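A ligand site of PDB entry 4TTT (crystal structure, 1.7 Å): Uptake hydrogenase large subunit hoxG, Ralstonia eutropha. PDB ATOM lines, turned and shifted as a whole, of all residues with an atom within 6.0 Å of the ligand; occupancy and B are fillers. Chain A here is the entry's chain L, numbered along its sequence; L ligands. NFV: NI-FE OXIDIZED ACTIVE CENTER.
The side-chain sulfur (SG) of Cys 75 lies close to the backbone NH (N) of Val 77, 3.4 Å away. The backbone NH of Cys 597 sits at hydrogen-bond distance from the side-chain hydroxyl of Thr 553. The side-chain sulfur of Cys 597 lies close to the side-chain carboxylate of Glu 27 (3.3 Å). The side-chain sulfur of Cys 600 lies close to a ring nitrogen (NE2) of His 82. The backbone carbonyl oxygen (O) of Cys 78 is in hydrogen-bond range of the side-chain sulfur (SG) of Cys 81 (3.3 Å). NH1 of Arg 530 lies within salt-bridge range of OD2 of Asp 117, at 2.8 Å. The guanidinium group (NH2) of Arg 530 is in salt-bridge range of the side-chain carboxylate (OD1) of Asp 595 (2.9 Å). O of Val 551 sits close to OG1 of Thr 554 (3.2 Å).
The side-chain sulfur (SG) of Cys 75 is bound to a nickel atom (NI) of the ligand, 2.2 Å away. SG of Cys 597 binds NI of the ligand, 2.2 Å away. An iron atom (FE) of the ligand is bound by the side-chain sulfur (SG) of Cys 600, at 2.3 Å. The side-chain sulfur (SG) of Cys 78 is bound to an iron atom (FE) of the ligand (2.4 Å). The backbone NH (N) of Arg 530 lies within hydrogen-bond range of a nitrogen (N3) of the ligand (2.9 Å). N3 of the ligand lies within hydrogen-bond range of NH1 of Arg 530. N of Thr 553 lies within hydrogen-bond range of N2 of the ligand (3.0 Å). The side-chain hydroxyl of Thr 553 is in hydrogen-bond range of a nitrogen (N2) of the ligand, at 2.9 Å. The side-chain sulfur of Cys 81 sits at hydrogen-bond distance from an oxygen (O1) of the ligand, at 3.4 Å. An oxygen (O1) of the ligand sits close to a ring nitrogen (NE2) of His 82 (3.5 Å).
N3 of the ligand lies close to N of Pro 529 (3.2 Å). Residues that only touch the ligand: Leu 533 (3.1 Å), Pro 552 (3.3 Å), Val 551 (3.5 Å) and Ala 528 (3.5 Å). Along chain A the residues within 4 Å of the ligand span positions 75 to 600. The nearest printed residue that does not touch the ligand is Val 77 (4.4 Å).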
ATOM      1  N   GLU A  27      30.390 -14.814  -3.433  1.00  0.00           N
ATOM      2  CA  GLU A  27      29.882 -16.078  -2.914  1.00  0.00           C
ATOM      3  C   GLU A  27      29.559 -16.957  -4.124  1.00  0.00           C
ATOM      4  O   GLU A  27      28.959 -16.497  -5.101  1.00  0.00           O
ATOM      5  CB  GLU A  27      28.645 -15.859  -2.038  1.00  0.00           C
ATOM      6  CG  GLU A  27      28.167 -17.100  -1.289  1.00  0.00           C
ATOM      7  CD  GLU A  27      27.620 -18.177  -2.215  1.00  0.00           C
ATOM      8  OE1 GLU A  27      27.017 -17.821  -3.244  1.00  0.00           O
ATOM      9  OE2 GLU A  27      27.809 -19.377  -1.915  1.00  0.00           O
ATOM     10  N   ILE A  74      20.172 -21.939   1.506  1.00  0.00           N
ATOM     11  CA  ILE A  74      20.491 -21.341   0.209  1.00  0.00           C
ATOM     12  C   ILE A  74      21.806 -20.565   0.301  1.00  0.00           C
ATOM     13  O   ILE A  74      22.604 -20.576  -0.642  1.00  0.00           O
ATOM     14  CB  ILE A  74      19.353 -20.431  -0.297  1.00  0.00           C
ATOM     15  CG1 ILE A  74      18.191 -21.309  -0.765  1.00  0.00           C
ATOM     16  CG2 ILE A  74      19.818 -19.547  -1.454  1.00  0.00           C
ATOM     17  CD1 ILE A  74      16.932 -20.546  -1.111  1.00  0.00           C
ATOM     18  N   CYS A  75      22.035 -19.902   1.433  1.00  0.00           N
ATOM     19  CA  CYS A  75      23.190 -19.039   1.573  1.00  0.00           C
ATOM     20  C   CYS A  75      23.618 -18.761   3.012  1.00  0.00           C
ATOM     21  O   CYS A  75      22.824 -18.304   3.831  1.00  0.00           O
ATOM     22  CB  CYS A  75      22.913 -17.714   0.878  1.00  0.00           C
ATOM     23  SG  CYS A  75      24.407 -16.720   0.677  1.00  0.00           S
ATOM     24  N   GLY A  76      24.902 -18.991   3.267  1.00  0.00           N
ATOM     25  CA  GLY A  76      25.519 -18.707   4.560  1.00  0.00           C
ATOM     26  C   GLY A  76      26.088 -17.301   4.673  1.00  0.00           C
ATOM     27  O   GLY A  76      26.509 -16.904   5.752  1.00  0.00           O
ATOM     28  N   VAL A  77      26.130 -16.564   3.565  1.00  0.00           N
ATOM     29  CA  VAL A  77      26.617 -15.191   3.571  1.00  0.00           C
ATOM     30  C   VAL A  77      25.457 -14.278   3.957  1.00  0.00           C
ATOM     31  O   VAL A  77      25.508 -13.584   4.992  1.00  0.00           O
ATOM     32  CB  VAL A  77      27.258 -14.794   2.217  1.00  0.00           C
ATOM     33  CG1 VAL A  77      27.686 -13.329   2.220  1.00  0.00           C
ATOM     34  CG2 VAL A  77      28.467 -15.681   1.921  1.00  0.00           C
ATOM     35  N   CYS A  78      24.384 -14.305   3.185  1.00  0.00           N
ATOM     36  CA  CYS A  78      23.171 -13.587   3.562  1.00  0.00           C
ATOM     37  C   CYS A  78      22.333 -14.456   4.503  1.00  0.00           C
ATOM     38  O   CYS A  78      21.158 -14.713   4.273  1.00  0.00           O
ATOM     39  CB  CYS A  78      22.377 -13.122   2.342  1.00  0.00           C
ATOM     40  SG  CYS A  78      21.860 -14.424   1.199  1.00  0.00           S
ATOM     41  N   THR A  79      22.969 -14.886   5.590  1.00  0.00           N
ATOM     42  CA  THR A  79      22.398 -15.919   6.442  1.00  0.00           C
ATOM     43  C   THR A  79      21.181 -15.418   7.238  1.00  0.00           C
ATOM     44  O   THR A  79      21.271 -14.410   7.953  1.00  0.00           O
ATOM     45  CB  THR A  79      23.444 -16.570   7.377  1.00  0.00           C
ATOM     46  OG1 THR A  79      22.822 -17.607   8.138  1.00  0.00           O
ATOM     47  CG2 THR A  79      24.102 -15.578   8.336  1.00  0.00           C
ATOM     48  N   CYS A  81      18.219 -14.347   5.901  1.00  0.00           N
ATOM     49  CA  CYS A  81      17.260 -13.559   5.116  1.00  0.00           C
ATOM     50  C   CYS A  81      16.260 -14.465   4.384  1.00  0.00           C
ATOM     51  O   CYS A  81      15.085 -14.129   4.272  1.00  0.00           O
ATOM     52  CB  CYS A  81      17.969 -12.580   4.179  1.00  0.00           C
ATOM     53  SG  CYS A  81      18.693 -13.269   2.685  1.00  0.00           S
ATOM     54  N   HIS A  82      16.718 -15.638   3.962  1.00  0.00           N
ATOM     55  CA  HIS A  82      15.831 -16.661   3.406  1.00  0.00           C
ATOM     56  C   HIS A  82      14.885 -17.273   4.457  1.00  0.00           C
ATOM     57  O   HIS A  82      13.730 -17.575   4.139  1.00  0.00           O
ATOM     58  CB  HIS A  82      16.650 -17.764   2.729  1.00  0.00           C
ATOM     59  CG  HIS A  82      17.317 -17.320   1.462  1.00  0.00           C
ATOM     60  ND1 HIS A  82      16.611 -17.073   0.311  1.00  0.00           N
ATOM     61  CD2 HIS A  82      18.611 -17.084   1.165  1.00  0.00           C
ATOM     62  CE1 HIS A  82      17.440 -16.702  -0.648  1.00  0.00           C
ATOM     63  NE2 HIS A  82      18.663 -16.685  -0.142  1.00  0.00           N
ATOM     64  N   ASP A 117      26.986  -8.159   6.523  1.00  0.00           N
ATOM     65  CA  ASP A 117      27.127  -8.501   5.105  1.00  0.00           C
ATOM     66  C   ASP A 117      27.782  -7.347   4.330  1.00  0.00           C
ATOM     67  O   ASP A 117      28.770  -7.547   3.629  1.00  0.00           O
ATOM     68  CB  ASP A 117      25.742  -8.880   4.538  1.00  0.00           C
ATOM     69  CG  ASP A 117      25.822  -9.852   3.388  1.00  0.00           C
ATOM     70  OD1 ASP A 117      26.823  -9.824   2.638  1.00  0.00           O
ATOM     71  OD2 ASP A 117      24.875 -10.661   3.227  1.00  0.00           O
ATOM     72  N   ALA A 528      16.608  -7.988   1.239  1.00  0.00           N
ATOM     73  CA  ALA A 528      17.858  -8.649   1.583  1.00  0.00           C
ATOM     74  C   ALA A 528      19.056  -7.755   1.243  1.00  0.00           C
ATOM     75  O   ALA A 528      18.910  -6.789   0.483  1.00  0.00           O
ATOM     76  CB  ALA A 528      17.955  -9.981   0.877  1.00  0.00           C
ATOM     77  N   PRO A 529      20.239  -8.044   1.815  1.00  0.00           N
ATOM     78  CA  PRO A 529      21.410  -7.209   1.531  1.00  0.00           C
ATOM     79  C   PRO A 529      21.657  -6.849   0.058  1.00  0.00           C
ATOM     80  O   PRO A 529      21.989  -5.715  -0.210  1.00  0.00           O
ATOM     81  CB  PRO A 529      22.566  -8.022   2.111  1.00  0.00           C
ATOM     82  CG  PRO A 529      21.951  -8.721   3.268  1.00  0.00           C
ATOM     83  CD  PRO A 529      20.545  -9.058   2.840  1.00  0.00           C
ATOM     84  N   ARG A 530      21.398  -7.779  -0.863  1.00  0.00           N
ATOM     85  CA  ARG A 530      21.680  -7.591  -2.287  1.00  0.00           C
ATOM     86  C   ARG A 530      20.480  -7.133  -3.118  1.00  0.00           C
ATOM     87  O   ARG A 530      20.619  -6.944  -4.326  1.00  0.00           O
ATOM     88  CB  ARG A 530      22.265  -8.873  -2.866  1.00  0.00           C
ATOM     89  CG  ARG A 530      23.667  -9.130  -2.373  1.00  0.00           C
ATOM     90  CD  ARG A 530      24.069 -10.595  -2.396  1.00  0.00           C
ATOM     91  NE  ARG A 530      25.348 -10.770  -1.714  1.00  0.00           N
ATOM     92  CZ  ARG A 530      25.532 -10.858  -0.383  1.00  0.00           C
ATOM     93  NH1 ARG A 530      24.511 -10.841   0.465  1.00  0.00           N
ATOM     94  NH2 ARG A 530      26.759 -10.994   0.095  1.00  0.00           N
ATOM     95  N   GLY A 531      19.331  -6.954  -2.490  1.00  0.00           N
ATOM     96  CA  GLY A 531      18.135  -6.444  -3.168  1.00  0.00           C
ATOM     97  C   GLY A 531      16.839  -7.122  -2.798  1.00  0.00           C
ATOM     98  O   GLY A 531      16.600  -7.482  -1.640  1.00  0.00           O
ATOM     99  N   LEU A 533      14.150  -9.790  -2.364  1.00  0.00           N
ATOM    100  CA  LEU A 533      13.995 -11.226  -2.161  1.00  0.00           C
ATOM    101  C   LEU A 533      12.518 -11.571  -1.971  1.00  0.00           C
ATOM    102  O   LEU A 533      11.803 -10.914  -1.209  1.00  0.00           O
ATOM    103  CB  LEU A 533      14.787 -11.692  -0.931  1.00  0.00           C
ATOM    104  CG  LEU A 533      14.565 -13.150  -0.496  1.00  0.00           C
ATOM    105  CD1 LEU A 533      14.974 -14.152  -1.571  1.00  0.00           C
ATOM    106  CD2 LEU A 533      15.291 -13.461   0.801  1.00  0.00           C
ATOM    107  N   VAL A 551      15.450 -14.361  -6.083  1.00  0.00           N
ATOM    108  CA  VAL A 551      16.465 -13.895  -5.141  1.00  0.00           C
ATOM    109  C   VAL A 551      17.194 -12.686  -5.770  1.00  0.00           C
ATOM    110  O   VAL A 551      17.210 -12.552  -6.991  1.00  0.00           O
ATOM    111  CB  VAL A 551      17.379 -15.098  -4.789  1.00  0.00           C
ATOM    112  CG1 VAL A 551      18.376 -14.787  -3.718  1.00  0.00           C
ATOM    113  CG2 VAL A 551      16.548 -16.301  -4.365  1.00  0.00           C
ATOM    114  N   PRO A 552      17.747 -11.767  -4.953  1.00  0.00           N
ATOM    115  CA  PRO A 552      18.274 -10.536  -5.581  1.00  0.00           C
ATOM    116  C   PRO A 552      19.324 -10.753  -6.687  1.00  0.00           C
ATOM    117  O   PRO A 552      19.248 -10.132  -7.746  1.00  0.00           O
ATOM    118  CB  PRO A 552      18.880  -9.766  -4.416  1.00  0.00           C
ATOM    119  CG  PRO A 552      18.103 -10.243  -3.231  1.00  0.00           C
ATOM    120  CD  PRO A 552      17.772 -11.676  -3.481  1.00  0.00           C
ATOM    121  N   THR A 553      20.274 -11.657  -6.452  1.00  0.00           N
ATOM    122  CA  THR A 553      21.289 -11.932  -7.463  1.00  0.00           C
ATOM    123  C   THR A 553      20.666 -12.680  -8.661  1.00  0.00           C
ATOM    124  O   THR A 553      21.211 -12.633  -9.767  1.00  0.00           O
ATOM    125  CB  THR A 553      22.550 -12.638  -6.883  1.00  0.00           C
ATOM    126  OG1 THR A 553      23.052 -11.860  -5.800  1.00  0.00           O
ATOM    127  CG2 THR A 553      23.653 -12.762  -7.938  1.00  0.00           C
ATOM    128  N   THR A 554      19.516 -13.341  -8.477  1.00  0.00           N
ATOM    129  CA  THR A 554      18.752 -13.845  -9.644  1.00  0.00           C
ATOM    130  C   THR A 554      18.378 -12.667 -10.571  1.00  0.00           C
ATOM    131  O   THR A 554      18.575 -12.744 -11.786  1.00  0.00           O
ATOM    132  CB  THR A 554      17.464 -14.594  -9.251  1.00  0.00           C
ATOM    133  OG1 THR A 554      17.703 -15.476  -8.148  1.00  0.00           O
ATOM    134  CG2 THR A 554      16.929 -15.383 -10.422  1.00  0.00           C
ATOM    135  N   ASP A 595      27.807  -7.136  -5.330  1.00  0.00           N
ATOM    136  CA  ASP A 595      27.927  -8.094  -4.250  1.00  0.00           C
ATOM    137  C   ASP A 595      27.277  -9.428  -4.686  1.00  0.00           C
ATOM    138  O   ASP A 595      26.326  -9.894  -4.055  1.00  0.00           O
ATOM    139  CB  ASP A 595      27.300  -7.472  -3.002  1.00  0.00           C
ATOM    140  CG  ASP A 595      27.428  -8.293  -1.768  1.00  0.00           C
ATOM    141  OD1 ASP A 595      28.157  -9.304  -1.730  1.00  0.00           O
ATOM    142  OD2 ASP A 595      26.737  -7.915  -0.807  1.00  0.00           O
ATOM    143  N   PRO A 596      27.771 -10.027  -5.777  1.00  0.00           N
ATOM    144  CA  PRO A 596      27.111 -11.219  -6.287  1.00  0.00           C
ATOM    145  C   PRO A 596      27.136 -12.380  -5.306  1.00  0.00           C
ATOM    146  O   PRO A 596      28.176 -12.684  -4.721  1.00  0.00           O
ATOM    147  CB  PRO A 596      27.931 -11.565  -7.539  1.00  0.00           C
ATOM    148  CG  PRO A 596      28.592 -10.292  -7.906  1.00  0.00           C
ATOM    149  CD  PRO A 596      28.930  -9.680  -6.600  1.00  0.00           C
ATOM    150  N   CYS A 597      25.971 -13.002  -5.124  1.00  0.00           N
ATOM    151  CA  CYS A 597      25.873 -14.235  -4.360  1.00  0.00           C
ATOM    152  C   CYS A 597      25.252 -15.292  -5.261  1.00  0.00           C
ATOM    153  O   CYS A 597      24.061 -15.264  -5.547  1.00  0.00           O
ATOM    154  CB  CYS A 597      25.028 -14.020  -3.112  1.00  0.00           C
ATOM    155  SG  CYS A 597      24.987 -15.456  -2.030  1.00  0.00           S
ATOM    156  N   ALA A 599      25.148 -18.728  -5.096  1.00  0.00           N
ATOM    157  CA  ALA A 599      24.315 -19.730  -4.428  1.00  0.00           C
ATOM    158  C   ALA A 599      22.898 -19.203  -4.242  1.00  0.00           C
ATOM    159  O   ALA A 599      21.929 -19.895  -4.531  1.00  0.00           O
ATOM    160  CB  ALA A 599      24.919 -20.122  -3.093  1.00  0.00           C
ATOM    161  N   CYS A 600      22.784 -17.965  -3.774  1.00  0.00           N
ATOM    162  CA  CYS A 600      21.517 -17.260  -3.764  1.00  0.00           C
ATOM    163  C   CYS A 600      20.847 -17.221  -5.120  1.00  0.00           C
ATOM    164  O   CYS A 600      19.673 -17.529  -5.248  1.00  0.00           O
ATOM    165  CB  CYS A 600      21.684 -15.830  -3.261  1.00  0.00           C
ATOM    166  SG  CYS A 600      21.361 -15.665  -1.501  1.00  0.00           S
ATOM    167  N   SER A 601      21.597 -16.832  -6.146  1.00  0.00           N
ATOM    168  CA  SER A 601      21.000 -16.587  -7.458  1.00  0.00           C
ATOM    169  C   SER A 601      20.343 -17.829  -8.039  1.00  0.00           C
ATOM    170  O   SER A 601      19.352 -17.722  -8.755  1.00  0.00           O
ATOM    171  CB  SER A 601      22.032 -16.029  -8.451  1.00  0.00           C
ATOM    172  OG  SER A 601      22.948 -17.020  -8.855  1.00  0.00           O
HETATM  173 FE   NFV L   1      21.243 -13.454  -0.877  1.00  0.00          FE
HETATM  174 NI   NFV L   1      23.647 -14.961  -0.351  1.00  0.00          NI
HETATM  175  C1  NFV L   1      19.264 -13.359  -0.698  1.00  0.00           C
HETATM  176  O1  NFV L   1      18.098 -13.283  -0.612  1.00  0.00           O
HETATM  177  C2  NFV L   1      21.198 -12.860  -2.592  1.00  0.00           C
HETATM  178  N2  NFV L   1      21.134 -12.525  -3.687  1.00  0.00           N
HETATM  179  C3  NFV L   1      21.247 -11.672  -0.327  1.00  0.00           C
HETATM  180  N3  NFV L   1      21.263 -10.534  -0.005  1.00  0.00           N
HETATM  181  O4  NFV L   1      23.332 -13.188  -0.955  1.00  0.00           O
